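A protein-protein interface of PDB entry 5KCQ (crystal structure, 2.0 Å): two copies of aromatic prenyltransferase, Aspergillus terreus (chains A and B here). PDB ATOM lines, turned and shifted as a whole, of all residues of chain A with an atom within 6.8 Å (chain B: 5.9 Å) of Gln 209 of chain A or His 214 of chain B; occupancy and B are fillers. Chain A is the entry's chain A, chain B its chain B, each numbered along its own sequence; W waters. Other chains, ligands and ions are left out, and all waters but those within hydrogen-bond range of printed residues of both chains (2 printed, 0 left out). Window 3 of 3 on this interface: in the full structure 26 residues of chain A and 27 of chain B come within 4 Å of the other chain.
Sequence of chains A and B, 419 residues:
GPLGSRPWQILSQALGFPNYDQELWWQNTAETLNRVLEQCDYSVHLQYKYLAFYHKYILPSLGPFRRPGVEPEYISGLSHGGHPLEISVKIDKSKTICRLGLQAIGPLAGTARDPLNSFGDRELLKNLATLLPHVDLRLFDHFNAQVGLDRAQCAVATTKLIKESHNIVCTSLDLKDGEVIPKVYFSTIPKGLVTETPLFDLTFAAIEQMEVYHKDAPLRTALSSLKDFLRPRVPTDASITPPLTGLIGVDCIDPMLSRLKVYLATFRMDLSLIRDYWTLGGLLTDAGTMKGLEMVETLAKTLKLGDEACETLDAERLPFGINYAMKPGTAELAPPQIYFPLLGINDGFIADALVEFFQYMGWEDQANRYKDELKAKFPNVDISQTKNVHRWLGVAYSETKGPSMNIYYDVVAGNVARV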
ATOM      1  N   HIS A 142      -8.672   1.881  -5.653  1.00  0.00           N
ATOM      2  CA  HIS A 142      -7.545   1.502  -6.468  1.00  0.00           C
ATOM      3  C   HIS A 142      -6.208   1.521  -5.746  1.00  0.00           C
ATOM      4  O   HIS A 142      -5.420   0.548  -5.749  1.00  0.00           O
ATOM      5  CB  HIS A 142      -7.478   2.414  -7.744  1.00  0.00           C
ATOM      6  CG  HIS A 142      -6.254   2.144  -8.541  1.00  0.00           C
ATOM      7  ND1 HIS A 142      -6.100   1.005  -9.286  1.00  0.00           N
ATOM      8  CD2 HIS A 142      -5.032   2.728  -8.502  1.00  0.00           C
ATOM      9  CE1 HIS A 142      -4.886   0.981  -9.795  1.00  0.00           C
ATOM     10  NE2 HIS A 142      -4.228   2.042  -9.358  1.00  0.00           N
ATOM     11  N   GLN A 146      -3.314  -1.220  -4.348  1.00  0.00           N
ATOM     12  CA  GLN A 146      -1.949  -1.297  -4.871  1.00  0.00           C
ATOM     13  C   GLN A 146      -0.895  -1.067  -3.820  1.00  0.00           C
ATOM     14  O   GLN A 146       0.186  -1.629  -3.880  1.00  0.00           O
ATOM     15  CB  GLN A 146      -1.682  -0.184  -5.878  1.00  0.00           C
ATOM     16  CG  GLN A 146      -2.616  -0.156  -7.048  1.00  0.00           C
ATOM     17  CD  GLN A 146      -2.725  -1.504  -7.713  1.00  0.00           C
ATOM     18  OE1 GLN A 146      -3.806  -2.130  -7.806  1.00  0.00           O
ATOM     19  NE2 GLN A 146      -1.595  -1.983  -8.134  1.00  0.00           N
ATOM     20  N   PHE A 204       5.058   4.279  -9.487  1.00  0.00           N
ATOM     21  CA  PHE A 204       4.621   4.267 -10.884  1.00  0.00           C
ATOM     22  C   PHE A 204       3.935   2.988 -11.303  1.00  0.00           C
ATOM     23  O   PHE A 204       3.016   3.058 -12.035  1.00  0.00           O
ATOM     24  CB  PHE A 204       5.791   4.735 -11.807  1.00  0.00           C
ATOM     25  CG  PHE A 204       6.037   6.225 -11.624  1.00  0.00           C
ATOM     26  CD1 PHE A 204       5.183   7.132 -12.199  1.00  0.00           C
ATOM     27  CD2 PHE A 204       7.024   6.700 -10.768  1.00  0.00           C
ATOM     28  CE1 PHE A 204       5.315   8.501 -11.974  1.00  0.00           C
ATOM     29  CE2 PHE A 204       7.168   8.051 -10.548  1.00  0.00           C
ATOM     30  CZ  PHE A 204       6.325   8.950 -11.158  1.00  0.00           C
ATOM     31  N   ALA A 205       4.280   1.820 -10.742  1.00  0.00           N
ATOM     32  CA  ALA A 205       3.503   0.625 -11.102  1.00  0.00           C
ATOM     33  C   ALA A 205       2.043   0.761 -10.665  1.00  0.00           C
ATOM     34  O   ALA A 205       1.130   0.390 -11.411  1.00  0.00           O
ATOM     35  CB  ALA A 205       4.110  -0.614 -10.501  1.00  0.00           C
ATOM     36  N   ALA A 206       1.805   1.325  -9.463  1.00  0.00           N
ATOM     37  CA  ALA A 206       0.444   1.515  -8.972  1.00  0.00           C
ATOM     38  C   ALA A 206      -0.311   2.517  -9.872  1.00  0.00           C
ATOM     39  O   ALA A 206      -1.494   2.337 -10.198  1.00  0.00           O
ATOM     40  CB  ALA A 206       0.461   2.056  -7.536  1.00  0.00           C
ATOM     41  N   ILE A 207       0.353   3.600 -10.196  1.00  0.00           N
ATOM     42  CA  ILE A 207      -0.247   4.607 -11.086  1.00  0.00           C
ATOM     43  C   ILE A 207      -0.558   4.011 -12.464  1.00  0.00           C
ATOM     44  O   ILE A 207      -1.652   4.195 -12.994  1.00  0.00           O
ATOM     45  CB  ILE A 207       0.633   5.867 -11.164  1.00  0.00           C
ATOM     46  CG1 ILE A 207       0.557   6.626  -9.835  1.00  0.00           C
ATOM     47  CG2 ILE A 207       0.167   6.717 -12.346  1.00  0.00           C
ATOM     48  CD1 ILE A 207       1.689   7.645  -9.691  1.00  0.00           C
ATOM     49  N   GLU A 208       0.354   3.212 -12.991  1.00  0.00           N
ATOM     50  CA  GLU A 208       0.179   2.697 -14.324  1.00  0.00           C
ATOM     51  C   GLU A 208      -0.944   1.660 -14.439  1.00  0.00           C
ATOM     52  O   GLU A 208      -1.412   1.379 -15.522  1.00  0.00           O
ATOM     53  CB  GLU A 208       1.533   2.147 -14.843  1.00  0.00           C
ATOM     54  CG  GLU A 208       2.483   3.351 -15.066  1.00  0.00           C
ATOM     55  CD  GLU A 208       3.934   2.969 -15.299  1.00  0.00           C
ATOM     56  OE1 GLU A 208       4.201   1.792 -15.525  1.00  0.00           O
ATOM     57  OE2 GLU A 208       4.803   3.846 -15.230  1.00  0.00           O
ATOM     58  N   GLN A 209      -1.417   1.151 -13.310  1.00  0.00           N
ATOM     59  CA  GLN A 209      -2.543   0.213 -13.327  1.00  0.00           C
ATOM     60  C   GLN A 209      -3.898   0.889 -13.161  1.00  0.00           C
ATOM     61  O   GLN A 209      -4.915   0.202 -13.091  1.00  0.00           O
ATOM     62  CB  GLN A 209      -2.296  -0.907 -12.268  1.00  0.00           C
ATOM     63  CG  GLN A 209      -1.237  -1.949 -12.747  1.00  0.00           C
ATOM     64  CD  GLN A 209      -0.289  -2.481 -11.656  1.00  0.00           C
ATOM     65  OE1 GLN A 209       0.885  -2.853 -11.936  1.00  0.00           O
ATOM     66  NE2 GLN A 209      -0.771  -2.541 -10.428  1.00  0.00           N
ATOM     67  N   MET A 210      -3.932   2.196 -13.006  1.00  0.00           N
ATOM     68  CA  MET A 210      -5.172   2.912 -12.889  1.00  0.00           C
ATOM     69  C   MET A 210      -5.993   2.720 -14.155  1.00  0.00           C
ATOM     70  O   MET A 210      -5.421   2.770 -15.278  1.00  0.00           O
ATOM     71  CB  MET A 210      -4.944   4.437 -12.735  1.00  0.00           C
ATOM     72  CG  MET A 210      -4.398   4.927 -11.403  1.00  0.00           C
ATOM     73  SD  MET A 210      -3.831   6.654 -11.602  1.00  0.00           S
ATOM     74  CE  MET A 210      -5.323   7.569 -11.375  1.00  0.00           C
ATOM     75  N   GLU A 211      -7.319   2.604 -14.013  1.00  0.00           N
ATOM     76  CA  GLU A 211      -8.229   2.550 -15.182  1.00  0.00           C
ATOM     77  C   GLU A 211      -8.083   3.791 -16.073  1.00  0.00           C
ATOM     78  O   GLU A 211      -7.970   3.685 -17.290  1.00  0.00           O
ATOM     79  CB  GLU A 211      -9.697   2.438 -14.744  1.00  0.00           C
ATOM     80  CG  GLU A 211     -10.636   2.215 -15.917  1.00  0.00           C
ATOM     81  CD  GLU A 211     -12.075   1.985 -15.467  1.00  0.00           C
ATOM     82  OE1 GLU A 211     -13.014   2.218 -16.215  1.00  0.00           O
ATOM     83  OE2 GLU A 211     -12.275   1.559 -14.331  1.00  0.00           O
ATOM     84  N   VAL A 212      -8.052   4.967 -15.450  1.00  0.00           N
ATOM     85  CA  VAL A 212      -7.899   6.236 -16.161  1.00  0.00           C
ATOM     86  C   VAL A 212      -6.578   6.410 -16.904  1.00  0.00           C
ATOM     87  O   VAL A 212      -6.569   6.994 -17.999  1.00  0.00           O
ATOM     88  CB  VAL A 212      -8.151   7.424 -15.231  1.00  0.00           C
ATOM     89  CG1 VAL A 212      -7.751   8.717 -15.901  1.00  0.00           C
ATOM     90  CG2 VAL A 212      -9.618   7.489 -14.896  1.00  0.00           C
ATOM     91  N   TYR A 213      -5.497   5.832 -16.377  1.00  0.00           N
ATOM     92  CA  TYR A 213      -4.217   5.821 -17.066  1.00  0.00           C
ATOM     93  C   TYR A 213      -4.375   5.002 -18.401  1.00  0.00           C
ATOM     94  O   TYR A 213      -3.878   5.433 -19.457  1.00  0.00           O
ATOM     95  CB  TYR A 213      -3.136   5.184 -16.172  1.00  0.00           C
ATOM     96  CG  TYR A 213      -1.763   5.026 -16.775  1.00  0.00           C
ATOM     97  CD1 TYR A 213      -1.433   3.920 -17.585  1.00  0.00           C
ATOM     98  CD2 TYR A 213      -0.791   5.980 -16.517  1.00  0.00           C
ATOM     99  CE1 TYR A 213      -0.178   3.808 -18.157  1.00  0.00           C
ATOM    100  CE2 TYR A 213       0.469   5.877 -17.047  1.00  0.00           C
ATOM    101  CZ  TYR A 213       0.776   4.825 -17.880  1.00  0.00           C
ATOM    102  OH  TYR A 213       2.041   4.728 -18.349  1.00  0.00           O
ATOM    103  N   HIS A 214      -5.011   3.817 -18.332  1.00  0.00           N
ATOM    104  CA  HIS A 214      -5.281   3.009 -19.526  1.00  0.00           C
ATOM    105  C   HIS A 214      -6.141   3.690 -20.621  1.00  0.00           C
ATOM    106  O   HIS A 214      -5.937   3.387 -21.769  1.00  0.00           O
ATOM    107  CB  HIS A 214      -5.870   1.656 -19.163  1.00  0.00           C
ATOM    108  CG  HIS A 214      -4.853   0.727 -18.608  1.00  0.00           C
ATOM    109  ND1 HIS A 214      -4.319  -0.308 -19.340  1.00  0.00           N
ATOM    110  CD2 HIS A 214      -4.194   0.728 -17.419  1.00  0.00           C
ATOM    111  CE1 HIS A 214      -3.417  -0.945 -18.607  1.00  0.00           C
ATOM    112  NE2 HIS A 214      -3.301  -0.315 -17.449  1.00  0.00           N
ATOM    113  N   HIS B 142      -9.498  -3.798  -5.443  1.00  0.00           N
ATOM    114  CA  HIS B 142      -9.198  -3.722  -6.885  1.00  0.00           C
ATOM    115  C   HIS B 142     -10.463  -3.775  -7.749  1.00  0.00           C
ATOM    116  O   HIS B 142     -10.782  -2.855  -8.559  1.00  0.00           O
ATOM    117  CB  HIS B 142      -8.228  -4.838  -7.276  1.00  0.00           C
ATOM    118  CG  HIS B 142      -8.005  -4.866  -8.750  1.00  0.00           C
ATOM    119  ND1 HIS B 142      -7.196  -3.961  -9.382  1.00  0.00           N
ATOM    120  CD2 HIS B 142      -8.660  -5.531  -9.721  1.00  0.00           C
ATOM    121  CE1 HIS B 142      -7.287  -4.130 -10.689  1.00  0.00           C
ATOM    122  NE2 HIS B 142      -8.196  -5.054 -10.925  1.00  0.00           N
ATOM    123  N   GLN B 146     -12.685  -1.065 -10.175  1.00  0.00           N
ATOM    124  CA  GLN B 146     -12.857  -1.237 -11.609  1.00  0.00           C
ATOM    125  C   GLN B 146     -14.311  -1.346 -11.990  1.00  0.00           C
ATOM    126  O   GLN B 146     -14.678  -0.898 -13.057  1.00  0.00           O
ATOM    127  CB  GLN B 146     -12.186  -2.539 -12.089  1.00  0.00           C
ATOM    128  CG  GLN B 146     -10.737  -2.685 -11.723  1.00  0.00           C
ATOM    129  CD  GLN B 146      -9.930  -1.490 -12.142  1.00  0.00           C
ATOM    130  OE1 GLN B 146      -9.223  -0.841 -11.333  1.00  0.00           O
ATOM    131  NE2 GLN B 146     -10.010  -1.205 -13.418  1.00  0.00           N
ATOM    132  N   GLU B 208      -7.028  -7.389 -16.341  1.00  0.00           N
ATOM    133  CA  GLU B 208      -5.684  -7.112 -16.859  1.00  0.00           C
ATOM    134  C   GLU B 208      -4.989  -5.997 -16.082  1.00  0.00           C
ATOM    135  O   GLU B 208      -3.754  -5.880 -16.136  1.00  0.00           O
ATOM    136  CB  GLU B 208      -5.733  -6.845 -18.382  1.00  0.00           C
ATOM    137  CG  GLU B 208      -6.098  -8.147 -19.096  1.00  0.00           C
ATOM    138  CD  GLU B 208      -6.560  -8.024 -20.538  1.00  0.00           C
ATOM    139  OE1 GLU B 208      -6.907  -9.104 -21.126  1.00  0.00           O
ATOM    140  OE2 GLU B 208      -6.598  -6.889 -21.055  1.00  0.00           O
ATOM    141  N   GLN B 209      -5.755  -5.230 -15.300  1.00  0.00           N
ATOM    142  CA  GLN B 209      -5.170  -4.208 -14.431  1.00  0.00           C
ATOM    143  C   GLN B 209      -4.824  -4.722 -13.030  1.00  0.00           C
ATOM    144  O   GLN B 209      -4.300  -3.964 -12.203  1.00  0.00           O
ATOM    145  CB  GLN B 209      -6.113  -2.980 -14.389  1.00  0.00           C
ATOM    146  CG  GLN B 209      -6.046  -2.134 -15.685  1.00  0.00           C
ATOM    147  CD  GLN B 209      -7.350  -1.468 -16.124  1.00  0.00           C
ATOM    148  OE1 GLN B 209      -8.148  -0.990 -15.310  1.00  0.00           O
ATOM    149  NE2 GLN B 209      -7.549  -1.384 -17.456  1.00  0.00           N
ATOM    150  N   MET B 210      -5.097  -5.994 -12.721  1.00  0.00           N
ATOM    151  CA  MET B 210      -4.686  -6.544 -11.441  1.00  0.00           C
ATOM    152  C   MET B 210      -3.164  -6.534 -11.299  1.00  0.00           C
ATOM    153  O   MET B 210      -2.441  -6.874 -12.277  1.00  0.00           O
ATOM    154  CB  MET B 210      -5.132  -7.985 -11.343  1.00  0.00           C
ATOM    155  CG  MET B 210      -6.624  -8.241 -11.176  1.00  0.00           C
ATOM    156  SD  MET B 210      -6.921 -10.032 -11.427  1.00  0.00           S
ATOM    157  CE  MET B 210      -6.545 -10.721  -9.846  1.00  0.00           C
ATOM    158  N   GLU B 211      -2.670  -6.286 -10.081  1.00  0.00           N
ATOM    159  CA  GLU B 211      -1.235  -6.345  -9.779  1.00  0.00           C
ATOM    160  C   GLU B 211      -0.673  -7.723 -10.087  1.00  0.00           C
ATOM    161  O   GLU B 211       0.395  -7.851 -10.702  1.00  0.00           O
ATOM    162  CB  GLU B 211      -0.919  -5.980  -8.309  1.00  0.00           C
ATOM    163  CG  GLU B 211       0.587  -5.866  -7.984  1.00  0.00           C
ATOM    164  CD  GLU B 211       0.875  -5.383  -6.575  1.00  0.00           C
ATOM    165  OE1 GLU B 211      -0.119  -5.129  -5.909  1.00  0.00           O
ATOM    166  OE2 GLU B 211       2.043  -5.253  -6.084  1.00  0.00           O
ATOM    167  N   VAL B 212      -1.371  -8.749  -9.642  1.00  0.00           N
ATOM    168  CA  VAL B 212      -0.920 -10.122  -9.839  1.00  0.00           C
ATOM    169  C   VAL B 212      -0.845 -10.580 -11.307  1.00  0.00           C
ATOM    170  O   VAL B 212      -0.008 -11.399 -11.629  1.00  0.00           O
ATOM    171  CB  VAL B 212      -1.735 -11.139  -9.038  1.00  0.00           C
ATOM    172  CG1 VAL B 212      -1.610 -10.865  -7.551  1.00  0.00           C
ATOM    173  CG2 VAL B 212      -3.208 -11.103  -9.425  1.00  0.00           C
ATOM    174  N   TYR B 213      -1.734 -10.070 -12.149  1.00  0.00           N
ATOM    175  CA  TYR B 213      -1.697 -10.315 -13.585  1.00  0.00           C
ATOM    176  C   TYR B 213      -0.372  -9.762 -14.146  1.00  0.00           C
ATOM    177  O   TYR B 213       0.305 -10.425 -14.935  1.00  0.00           O
ATOM    178  CB  TYR B 213      -2.889  -9.604 -14.255  1.00  0.00           C
ATOM    179  CG  TYR B 213      -2.942  -9.704 -15.765  1.00  0.00           C
ATOM    180  CD1 TYR B 213      -2.202  -8.829 -16.584  1.00  0.00           C
ATOM    181  CD2 TYR B 213      -3.724 -10.679 -16.381  1.00  0.00           C
ATOM    182  CE1 TYR B 213      -2.259  -8.931 -17.984  1.00  0.00           C
ATOM    183  CE2 TYR B 213      -3.799 -10.788 -17.745  1.00  0.00           C
ATOM    184  CZ  TYR B 213      -3.060  -9.940 -18.551  1.00  0.00           C
ATOM    185  OH  TYR B 213      -3.185 -10.096 -19.900  1.00  0.00           O
ATOM    186  N   HIS B 214      -0.013  -8.544 -13.746  1.00  0.00           N
ATOM    187  CA  HIS B 214       1.299  -7.980 -14.129  1.00  0.00           C
ATOM    188  C   HIS B 214       2.533  -8.778 -13.686  1.00  0.00           C
ATOM    189  O   HIS B 214       3.543  -8.736 -14.342  1.00  0.00           O
ATOM    190  CB  HIS B 214       1.410  -6.527 -13.692  1.00  0.00           C
ATOM    191  CG  HIS B 214       0.622  -5.614 -14.557  1.00  0.00           C
ATOM    192  ND1 HIS B 214       1.205  -4.831 -15.533  1.00  0.00           N
ATOM    193  CD2 HIS B 214      -0.717  -5.411 -14.651  1.00  0.00           C
ATOM    194  CE1 HIS B 214       0.257  -4.149 -16.162  1.00  0.00           C
ATOM    195  NE2 HIS B 214      -0.917  -4.487 -15.649  1.00  0.00           N
ATOM    196  N   LYS B 215       2.445  -9.515 -12.607  1.00  0.00           N
ATOM    197  CA  LYS B 215       3.547 -10.323 -12.108  1.00  0.00           C
ATOM    198  C   LYS B 215       3.525 -11.790 -12.508  1.00  0.00           C
ATOM    199  O   LYS B 215       4.499 -12.496 -12.276  1.00  0.00           O
ATOM    200  CB  LYS B 215       3.486 -10.356 -10.582  1.00  0.00           C
ATOM    201  CG  LYS B 215       3.647  -9.021  -9.885  1.00  0.00           C
ATOM    202  CD  LYS B 215       3.360  -9.153  -8.394  1.00  0.00           C
ATOM    203  CE  LYS B 215       4.437  -9.976  -7.694  1.00  0.00           C
ATOM    204  NZ  LYS B 215       4.292  -9.863  -6.225  1.00  0.00           N
ATOM    205  N   ASP B 216       2.401 -12.301 -12.997  1.00  0.00           N
ATOM    206  CA  ASP B 216       2.280 -13.754 -13.174  1.00  0.00           C
ATOM    207  C   ASP B 216       2.016 -14.194 -14.621  1.00  0.00           C
ATOM    208  O   ASP B 216       0.903 -14.141 -15.119  1.00  0.00           O
ATOM    209  CB  ASP B 216       1.207 -14.308 -12.232  1.00  0.00           C
ATOM    210  CG  ASP B 216       1.337 -15.806 -12.052  1.00  0.00           C
ATOM    211  OD1 ASP B 216       2.252 -16.200 -11.335  1.00  0.00           O
ATOM    212  OD2 ASP B 216       0.561 -16.586 -12.657  1.00  0.00           O
ATOM    213  N   ARG B 220      -1.548 -14.909 -17.047  1.00  0.00           N
ATOM    214  CA  ARG B 220      -1.788 -14.210 -18.292  1.00  0.00           C
ATOM    215  C   ARG B 220      -2.013 -15.219 -19.450  1.00  0.00           C
ATOM    216  O   ARG B 220      -2.814 -14.973 -20.306  1.00  0.00           O
ATOM    217  CB  ARG B 220      -0.639 -13.274 -18.628  1.00  0.00           C
ATOM    218  CG  ARG B 220      -0.350 -12.171 -17.617  1.00  0.00           C
ATOM    219  CD  ARG B 220       0.475 -11.049 -18.259  1.00  0.00           C
ATOM    220  NE  ARG B 220       1.865 -11.466 -18.539  1.00  0.00           N
ATOM    221  CZ  ARG B 220       2.830 -11.582 -17.619  1.00  0.00           C
ATOM    222  NH1 ARG B 220       2.592 -11.284 -16.359  1.00  0.00           N
ATOM    223  NH2 ARG B 220       4.060 -11.967 -17.966  1.00  0.00           N
HETATM  224  O   HOH W   1      -4.671  -4.961  -8.220  1.00  0.00           O
HETATM  225  O   HOH W   2      -8.408   2.049 -11.383  1.00  0.00           O
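Gln 209 of chain B touches its own counterpart, Gln 209 of chain A.
Gln 209 of chain A touches Glu 211 of chain B, and with the chains exchanged Glu 211 of chain A touches Gln 209 of chain B.
Gln 209 of chain A touches His 214 of chain B, and with the chains exchanged His 214 of chain A touches Gln 209 of chain B.
Glu 211 of chain A touches Gln 146 of chain B, but with the chains exchanged Gln 146 of chain A does not touch Glu 211 of chain B (4.1 Å).
Of the 12 printed residues of chain B, 4 touch a printed residue of chain A.
Hydrophobic or aromatic side chains of chain B that line the printed part of chain A: His 214.
Along chain B the printed residues that touch a printed residue of chain A span positions 146 to 214.
Hydrophobic or aromatic side chains of chain A that line the printed part of chain B: His 214.
Among the printed residues, no Asp or Glu carboxylate lies within 4 Å of a Lys or Arg side-chain nitrogen of the other chain.
Water W2 lies within hydrogen-bond range of N of Glu 211 of chain A, OE1 of Gln 146 of chain B and ND1 of His 142 of chain A.
Water W1 lies within hydrogen-bond range of a ring nitrogen (ND1) of His 142 of chain B (3.0 Å), the side-chain amide oxygen (OE1) of Gln 146 of chain A (3.0 Å) and the backbone NH (N) of Glu 211 of chain B (3.0 Å).
Printed residues of chain B within 4 Å of Gln 209 of chain A: Gln 209 (3.6 Å), Glu 211 (3.9 Å) and His 214 (3.8 Å).
Of the printed residues of chain A, His 214 of chain B touches Gln 209 (3.8 Å).
Of the printed residues of chain B, His 214 of chain A touches Gln 209.
Printed residues of chain A within 4 Å of Gln 209 of chain B: Gln 209, Glu 211 and His 214.
Of the printed residues of chain A, Gln 146 of chain B touches Glu 211.
Asp 216 of chain B touches none of the printed residues of chain A.
The nearest printed residue of chain A that does not touch Gln 146 of chain B is His 142 of chain A (4.2 Å).
O of Gln 209 of chain A touches CB of Gln 209 of chain B, 3.6 Å away.
Gln 209 of chain A touches Glu 211 of chain B.
Gln 209 of chain A touches His 214 of chain B.
OE2 of Glu 211 of chain A touches O of Gln 146 of chain B (3.7 Å).
Glu 211 of chain A touches Gln 209 of chain B (CA to OE1, 3.5 Å).
His 214 of chain A touches Gln 209 of chain B.
The backbone carbonyl oxygen (O) of His 214 of chain B lies within hydrogen-bond range of the guanidinium group (NH1) of Arg 220 of chain B (3.4 Å).
The side-chain amide oxygen of Gln 209 of chain B is in hydrogen-bond range of the side-chain amide nitrogen of Gln 146 of chain B (2.7 Å).
O of Ala 205 of chain A sits close to OE1 of Gln 209 of chain A (3.3 Å).
A ring nitrogen (NE2) of His 214 of chain A sits at hydrogen-bond distance from the backbone carbonyl oxygen (O) of Glu 208 of chain A (3.2 Å).
The backbone carbonyl oxygen (O) of Glu 208 of chain B sits at hydrogen-bond distance from a ring nitrogen (NE2) of His 214 of chain B, 3.2 Å away.
NE2 of Gln 209 of chain A lies close to NE2 of Gln 146 of chain A (2.5 Å).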
